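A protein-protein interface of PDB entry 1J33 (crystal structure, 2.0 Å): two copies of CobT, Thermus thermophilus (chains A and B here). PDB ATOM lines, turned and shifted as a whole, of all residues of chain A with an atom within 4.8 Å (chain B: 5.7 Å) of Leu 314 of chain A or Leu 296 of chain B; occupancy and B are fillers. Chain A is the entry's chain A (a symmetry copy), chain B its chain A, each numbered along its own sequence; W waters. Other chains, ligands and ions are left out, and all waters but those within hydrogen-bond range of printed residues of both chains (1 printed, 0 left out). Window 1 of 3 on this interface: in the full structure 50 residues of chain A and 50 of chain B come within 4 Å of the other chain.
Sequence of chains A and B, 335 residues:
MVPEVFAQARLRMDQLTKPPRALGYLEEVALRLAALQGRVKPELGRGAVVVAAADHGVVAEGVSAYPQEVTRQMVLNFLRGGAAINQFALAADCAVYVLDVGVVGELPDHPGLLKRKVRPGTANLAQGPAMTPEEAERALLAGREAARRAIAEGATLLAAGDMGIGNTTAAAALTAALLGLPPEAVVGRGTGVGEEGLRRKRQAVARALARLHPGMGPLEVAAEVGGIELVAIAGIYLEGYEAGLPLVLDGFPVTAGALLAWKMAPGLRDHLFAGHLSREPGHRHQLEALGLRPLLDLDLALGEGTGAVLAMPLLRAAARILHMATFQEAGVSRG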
ATOM      1  N   LEU A  26      -4.259 -19.827 -17.071  1.00  0.00           N
ATOM      2  CA  LEU A  26      -4.997 -19.358 -18.232  1.00  0.00           C
ATOM      3  C   LEU A  26      -6.111 -18.417 -17.828  1.00  0.00           C
ATOM      4  O   LEU A  26      -6.608 -17.661 -18.652  1.00  0.00           O
ATOM      5  CB  LEU A  26      -5.588 -20.522 -19.030  1.00  0.00           C
ATOM      6  CG  LEU A  26      -4.591 -21.413 -19.770  1.00  0.00           C
ATOM      7  CD1 LEU A  26      -5.352 -22.362 -20.692  1.00  0.00           C
ATOM      8  CD2 LEU A  26      -3.632 -20.547 -20.585  1.00  0.00           C
ATOM      9  N   LEU A 295       4.315 -18.950 -20.842  1.00  0.00           N
ATOM     10  CA  LEU A 295       3.203 -19.848 -21.123  1.00  0.00           C
ATOM     11  C   LEU A 295       3.726 -21.246 -21.447  1.00  0.00           C
ATOM     12  O   LEU A 295       3.063 -22.242 -21.173  1.00  0.00           O
ATOM     13  CB  LEU A 295       2.387 -19.327 -22.309  1.00  0.00           C
ATOM     14  CG  LEU A 295       1.546 -18.082 -22.033  1.00  0.00           C
ATOM     15  CD1 LEU A 295       0.995 -17.532 -23.334  1.00  0.00           C
ATOM     16  CD2 LEU A 295       0.422 -18.443 -21.084  1.00  0.00           C
ATOM     17  N   LEU A 296       4.917 -21.305 -22.035  1.00  0.00           N
ATOM     18  CA  LEU A 296       5.531 -22.570 -22.409  1.00  0.00           C
ATOM     19  C   LEU A 296       6.965 -22.686 -21.913  1.00  0.00           C
ATOM     20  O   LEU A 296       7.655 -21.687 -21.735  1.00  0.00           O
ATOM     21  CB  LEU A 296       5.557 -22.710 -23.934  1.00  0.00           C
ATOM     22  CG  LEU A 296       4.234 -22.746 -24.691  1.00  0.00           C
ATOM     23  CD1 LEU A 296       4.483 -22.598 -26.183  1.00  0.00           C
ATOM     24  CD2 LEU A 296       3.526 -24.050 -24.390  1.00  0.00           C
ATOM     25  N   ALA A 311       2.882 -20.194 -28.894  1.00  0.00           N
ATOM     26  CA  ALA A 311       1.967 -19.852 -27.811  1.00  0.00           C
ATOM     27  C   ALA A 311       0.672 -19.178 -28.261  1.00  0.00           C
ATOM     28  O   ALA A 311      -0.280 -19.047 -27.475  1.00  0.00           O
ATOM     29  CB  ALA A 311       2.682 -18.963 -26.803  1.00  0.00           C
ATOM     30  N   MET A 312       0.609 -18.763 -29.520  1.00  0.00           N
ATOM     31  CA  MET A 312      -0.601 -18.088 -29.978  1.00  0.00           C
ATOM     32  C   MET A 312      -1.853 -18.932 -29.773  1.00  0.00           C
ATOM     33  O   MET A 312      -2.854 -18.431 -29.279  1.00  0.00           O
ATOM     34  CB  MET A 312      -0.452 -17.653 -31.435  1.00  0.00           C
ATOM     35  CG  MET A 312       0.525 -16.477 -31.597  1.00  0.00           C
ATOM     36  SD  MET A 312       0.648 -15.913 -33.303  1.00  0.00           S
ATOM     37  CE  MET A 312       1.718 -14.488 -33.145  1.00  0.00           C
ATOM     38  N   PRO A 313      -1.814 -20.226 -30.142  1.00  0.00           N
ATOM     39  CA  PRO A 313      -3.000 -21.064 -29.948  1.00  0.00           C
ATOM     40  C   PRO A 313      -3.491 -21.040 -28.497  1.00  0.00           C
ATOM     41  O   PRO A 313      -4.694 -21.026 -28.246  1.00  0.00           O
ATOM     42  CB  PRO A 313      -2.511 -22.444 -30.370  1.00  0.00           C
ATOM     43  CG  PRO A 313      -1.586 -22.111 -31.499  1.00  0.00           C
ATOM     44  CD  PRO A 313      -0.794 -20.946 -30.931  1.00  0.00           C
ATOM     45  N   LEU A 314      -2.554 -21.042 -27.547  1.00  0.00           N
ATOM     46  CA  LEU A 314      -2.902 -20.998 -26.128  1.00  0.00           C
ATOM     47  C   LEU A 314      -3.608 -19.693 -25.783  1.00  0.00           C
ATOM     48  O   LEU A 314      -4.583 -19.681 -25.033  1.00  0.00           O
ATOM     49  CB  LEU A 314      -1.658 -21.110 -25.254  1.00  0.00           C
ATOM     50  CG  LEU A 314      -0.896 -22.426 -25.227  1.00  0.00           C
ATOM     51  CD1 LEU A 314       0.098 -22.377 -24.080  1.00  0.00           C
ATOM     52  CD2 LEU A 314      -1.865 -23.585 -25.031  1.00  0.00           C
ATOM     53  N   LEU A 315      -3.097 -18.590 -26.316  1.00  0.00           N
ATOM     54  CA  LEU A 315      -3.699 -17.286 -26.064  1.00  0.00           C
ATOM     55  C   LEU A 315      -5.128 -17.253 -26.614  1.00  0.00           C
ATOM     56  O   LEU A 315      -6.020 -16.662 -26.007  1.00  0.00           O
ATOM     57  CB  LEU A 315      -2.850 -16.191 -26.706  1.00  0.00           C
ATOM     58  CG  LEU A 315      -1.447 -16.052 -26.108  1.00  0.00           C
ATOM     59  CD1 LEU A 315      -0.635 -15.081 -26.938  1.00  0.00           C
ATOM     60  CD2 LEU A 315      -1.547 -15.580 -24.660  1.00  0.00           C
ATOM     61  N   ARG A 316      -5.345 -17.896 -27.757  1.00  0.00           N
ATOM     62  CA  ARG A 316      -6.677 -17.949 -28.346  1.00  0.00           C
ATOM     63  C   ARG A 316      -7.573 -18.813 -27.463  1.00  0.00           C
ATOM     64  O   ARG A 316      -8.748 -18.513 -27.266  1.00  0.00           O
ATOM     65  CB  ARG A 316      -6.625 -18.543 -29.757  1.00  0.00           C
ATOM     66  CG  ARG A 316      -5.790 -17.745 -30.737  1.00  0.00           C
ATOM     67  CD  ARG A 316      -6.123 -18.127 -32.172  1.00  0.00           C
ATOM     68  NE  ARG A 316      -5.325 -17.370 -33.131  1.00  0.00           N
ATOM     69  CZ  ARG A 316      -4.203 -17.814 -33.688  1.00  0.00           C
ATOM     70  NH1 ARG A 316      -3.745 -19.024 -33.386  1.00  0.00           N
ATOM     71  NH2 ARG A 316      -3.533 -17.046 -34.539  1.00  0.00           N
ATOM     72  N   ALA A 317      -7.017 -19.895 -26.926  1.00  0.00           N
ATOM     73  CA  ALA A 317      -7.795 -20.764 -26.056  1.00  0.00           C
ATOM     74  C   ALA A 317      -8.154 -20.008 -24.775  1.00  0.00           C
ATOM     75  O   ALA A 317      -9.268 -20.131 -24.267  1.00  0.00           O
ATOM     76  CB  ALA A 317      -7.005 -22.030 -25.728  1.00  0.00           C
ATOM     77  N   ALA A 318      -7.209 -19.231 -24.248  1.00  0.00           N
ATOM     78  CA  ALA A 318      -7.467 -18.461 -23.034  1.00  0.00           C
ATOM     79  C   ALA A 318      -8.552 -17.423 -23.314  1.00  0.00           C
ATOM     80  O   ALA A 318      -9.419 -17.186 -22.482  1.00  0.00           O
ATOM     81  CB  ALA A 318      -6.196 -17.770 -22.566  1.00  0.00           C
ATOM     82  N   ALA B 274       1.708 -36.710 -23.146  1.00  0.00           N
ATOM     83  CA  ALA B 274       1.086 -36.041 -22.015  1.00  0.00           C
ATOM     84  C   ALA B 274       0.811 -34.584 -22.358  1.00  0.00           C
ATOM     85  O   ALA B 274       1.732 -33.789 -22.535  1.00  0.00           O
ATOM     86  CB  ALA B 274       1.984 -36.129 -20.790  1.00  0.00           C
ATOM     87  N   GLY B 275      -0.463 -34.233 -22.447  1.00  0.00           N
ATOM     88  CA  GLY B 275      -0.807 -32.863 -22.765  1.00  0.00           C
ATOM     89  C   GLY B 275      -0.328 -31.874 -21.718  1.00  0.00           C
ATOM     90  O   GLY B 275       0.149 -30.790 -22.057  1.00  0.00           O
ATOM     91  N   HIS B 276      -0.443 -32.245 -20.447  1.00  0.00           N
ATOM     92  CA  HIS B 276      -0.033 -31.352 -19.368  1.00  0.00           C
ATOM     93  C   HIS B 276       0.150 -32.070 -18.033  1.00  0.00           C
ATOM     94  O   HIS B 276      -0.097 -33.274 -17.909  1.00  0.00           O
ATOM     95  CB  HIS B 276      -1.083 -30.237 -19.183  1.00  0.00           C
ATOM     96  CG  HIS B 276      -2.382 -30.714 -18.600  1.00  0.00           C
ATOM     97  ND1 HIS B 276      -2.996 -30.085 -17.537  1.00  0.00           N
ATOM     98  CD2 HIS B 276      -3.176 -31.765 -18.920  1.00  0.00           C
ATOM     99  CE1 HIS B 276      -4.107 -30.728 -17.226  1.00  0.00           C
ATOM    100  NE2 HIS B 276      -4.240 -31.753 -18.049  1.00  0.00           N
ATOM    101  N   LEU B 277       0.613 -31.314 -17.043  1.00  0.00           N
ATOM    102  CA  LEU B 277       0.776 -31.824 -15.689  1.00  0.00           C
ATOM    103  C   LEU B 277      -0.262 -31.028 -14.900  1.00  0.00           C
ATOM    104  O   LEU B 277      -0.144 -29.813 -14.764  1.00  0.00           O
ATOM    105  CB  LEU B 277       2.176 -31.527 -15.143  1.00  0.00           C
ATOM    106  CG  LEU B 277       2.397 -31.972 -13.690  1.00  0.00           C
ATOM    107  CD1 LEU B 277       2.297 -33.487 -13.601  1.00  0.00           C
ATOM    108  CD2 LEU B 277       3.755 -31.505 -13.195  1.00  0.00           C
ATOM    109  N   PRO B 294       5.276 -33.840 -19.576  1.00  0.00           N
ATOM    110  CA  PRO B 294       4.116 -32.998 -19.893  1.00  0.00           C
ATOM    111  C   PRO B 294       4.495 -31.894 -20.869  1.00  0.00           C
ATOM    112  O   PRO B 294       5.529 -31.249 -20.705  1.00  0.00           O
ATOM    113  CB  PRO B 294       3.713 -32.416 -18.533  1.00  0.00           C
ATOM    114  CG  PRO B 294       4.383 -33.307 -17.531  1.00  0.00           C
ATOM    115  CD  PRO B 294       5.684 -33.659 -18.174  1.00  0.00           C
ATOM    116  N   LEU B 295       3.658 -31.677 -21.879  1.00  0.00           N
ATOM    117  CA  LEU B 295       3.912 -30.632 -22.861  1.00  0.00           C
ATOM    118  C   LEU B 295       3.568 -29.264 -22.274  1.00  0.00           C
ATOM    119  O   LEU B 295       4.175 -28.259 -22.630  1.00  0.00           O
ATOM    120  CB  LEU B 295       3.068 -30.869 -24.117  1.00  0.00           C
ATOM    121  CG  LEU B 295       3.502 -32.044 -24.990  1.00  0.00           C
ATOM    122  CD1 LEU B 295       2.451 -32.319 -26.046  1.00  0.00           C
ATOM    123  CD2 LEU B 295       4.836 -31.719 -25.631  1.00  0.00           C
ATOM    124  N   LEU B 296       2.587 -29.241 -21.376  1.00  0.00           N
ATOM    125  CA  LEU B 296       2.149 -28.006 -20.743  1.00  0.00           C
ATOM    126  C   LEU B 296       2.082 -28.125 -19.227  1.00  0.00           C
ATOM    127  O   LEU B 296       1.881 -29.208 -18.686  1.00  0.00           O
ATOM    128  CB  LEU B 296       0.749 -27.631 -21.240  1.00  0.00           C
ATOM    129  CG  LEU B 296       0.550 -27.334 -22.722  1.00  0.00           C
ATOM    130  CD1 LEU B 296      -0.934 -27.271 -23.046  1.00  0.00           C
ATOM    131  CD2 LEU B 296       1.232 -26.026 -23.061  1.00  0.00           C
ATOM    132  N   ASP B 297       2.248 -26.997 -18.549  1.00  0.00           N
ATOM    133  CA  ASP B 297       2.123 -26.955 -17.098  1.00  0.00           C
ATOM    134  C   ASP B 297       1.522 -25.591 -16.804  1.00  0.00           C
ATOM    135  O   ASP B 297       2.241 -24.609 -16.586  1.00  0.00           O
ATOM    136  CB  ASP B 297       3.466 -27.081 -16.386  1.00  0.00           C
ATOM    137  CG  ASP B 297       3.294 -27.294 -14.888  1.00  0.00           C
ATOM    138  OD1 ASP B 297       2.393 -26.657 -14.306  1.00  0.00           O
ATOM    139  OD2 ASP B 297       4.044 -28.091 -14.294  1.00  0.00           O
ATOM    140  N   LEU B 298       0.195 -25.541 -16.814  1.00  0.00           N
ATOM    141  CA  LEU B 298      -0.531 -24.301 -16.592  1.00  0.00           C
ATOM    142  C   LEU B 298      -1.372 -24.360 -15.320  1.00  0.00           C
ATOM    143  O   LEU B 298      -2.341 -23.618 -15.167  1.00  0.00           O
ATOM    144  CB  LEU B 298      -1.411 -24.026 -17.814  1.00  0.00           C
ATOM    145  CG  LEU B 298      -0.619 -23.919 -19.124  1.00  0.00           C
ATOM    146  CD1 LEU B 298      -1.529 -24.095 -20.342  1.00  0.00           C
ATOM    147  CD2 LEU B 298       0.071 -22.568 -19.158  1.00  0.00           C
ATOM    148  N   GLY B 307      -6.895 -30.194 -20.934  1.00  0.00           N
ATOM    149  CA  GLY B 307      -5.443 -30.164 -21.021  1.00  0.00           C
ATOM    150  C   GLY B 307      -4.900 -30.856 -22.261  1.00  0.00           C
ATOM    151  O   GLY B 307      -3.915 -30.413 -22.853  1.00  0.00           O
ATOM    152  N   LEU B 310      -5.744 -28.666 -25.347  1.00  0.00           N
ATOM    153  CA  LEU B 310      -4.903 -27.476 -25.415  1.00  0.00           C
ATOM    154  C   LEU B 310      -3.535 -27.785 -26.008  1.00  0.00           C
ATOM    155  O   LEU B 310      -2.900 -26.912 -26.598  1.00  0.00           O
ATOM    156  CB  LEU B 310      -4.729 -26.858 -24.031  1.00  0.00           C
ATOM    157  CG  LEU B 310      -5.895 -26.049 -23.459  1.00  0.00           C
ATOM    158  CD1 LEU B 310      -5.660 -25.803 -21.968  1.00  0.00           C
ATOM    159  CD2 LEU B 310      -6.005 -24.722 -24.207  1.00  0.00           C
ATOM    160  N   ALA B 311      -3.091 -29.031 -25.864  1.00  0.00           N
ATOM    161  CA  ALA B 311      -1.787 -29.439 -26.376  1.00  0.00           C
ATOM    162  C   ALA B 311      -1.790 -29.891 -27.835  1.00  0.00           C
ATOM    163  O   ALA B 311      -0.725 -30.041 -28.453  1.00  0.00           O
ATOM    164  CB  ALA B 311      -1.222 -30.548 -25.500  1.00  0.00           C
ATOM    165  N   LEU B 314       0.273 -27.828 -30.259  1.00  0.00           N
ATOM    166  CA  LEU B 314       1.706 -28.058 -30.082  1.00  0.00           C
ATOM    167  C   LEU B 314       2.147 -29.317 -30.816  1.00  0.00           C
ATOM    168  O   LEU B 314       3.201 -29.343 -31.450  1.00  0.00           O
ATOM    169  CB  LEU B 314       2.058 -28.219 -28.608  1.00  0.00           C
ATOM    170  CG  LEU B 314       1.939 -27.014 -27.689  1.00  0.00           C
ATOM    171  CD1 LEU B 314       2.619 -27.349 -26.373  1.00  0.00           C
ATOM    172  CD2 LEU B 314       2.607 -25.803 -28.329  1.00  0.00           C
HETATM  173  O   HOH W   1       3.511 -24.568 -19.954  1.00  0.00           O
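Of chain B, only Leu 296 and Leu 310 come within 4 Å of Leu 314 of chain A. Printed residues of chain B within 4 Å of Ala 317 of chain A: Leu 310 (3.2 Å). His 276 of chain B touches none of the printed residues of chain A. Pro 294 of chain B touches none of the printed residues of chain A. Of the printed residues of chain A, Leu 310 of chain B touches Leu 26 (3.7 Å), Leu 314 (3.8 Å) and Ala 317 (3.2 Å). The nearest residue of chain A that does not touch Leu 296 of chain B is Leu 295 of chain A (4.6 Å).
Water W1 lies within hydrogen-bond range of O of Leu 295 of chain A (2.7 Å) and N of Asp 297 of chain B (3.1 Å).
The backbone NH (N) of Leu 296 of chain B lies within hydrogen-bond range of the backbone carbonyl oxygen (O) of Gly 275 of chain B, 3.0 Å away. The backbone carbonyl oxygen (O) of Leu 296 of chain B sits at hydrogen-bond distance from the backbone NH (N) of Leu 277 of chain B (3.0 Å).
Of the 11 printed residues of chain A, 5 touch a printed residue of chain B. Printed residues of chain A that touch a printed residue of chain B: Leu 26, Leu 295, Leu 296, Leu 314 and Ala 317. Hydrophobic or aromatic side chains of chain A that line the printed part of chain B: Leu 26, Leu 296, Leu 314 and Ala 317. Of the 13 printed residues of chain B, 4 touch a printed residue of chain A. Along chain B the printed residues that touch a printed residue of chain A span positions 296 to 314. Among the printed residues, 7 pairs touch across the chains. Among the printed residues, no Asp or Glu carboxylate lies within 4 Å of a Lys or Arg side-chain nitrogen of the other chain.
Leu 296 of chain A touches its own counterpart, Leu 296 of chain B. Leu 296 of chain A touches Leu 314 of chain B, and with the chains exchanged Leu 314 of chain A touches Leu 296 of chain B. 4 positions are printed for both chains. Of the 7 pairs that touch across the chains among the printed residues, 3 have their exchanged pair printed and touching as well.
Leu 26 of chain A touches Leu 310 of chain B (CD1 to CD1, 3.7 Å). O of Leu 295 of chain A touches CD2 of Leu 298 of chain B, 3.6 Å away. Leu 296 of chain B touches Leu 296 of chain A (CD2 to CD2, 3.3 Å). CD2 of Leu 296 of chain A touches CD1 of Leu 314 of chain B (3.95 Å). CD1 of Leu 314 of chain A touches CD2 of Leu 296 of chain B (3.95 Å). O of Leu 310 of chain B touches CD2 of Leu 314 of chain A, 3.8 Å away. CB of Ala 317 of chain A touches CD2 of Leu 310 of chain B (3.2 Å).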
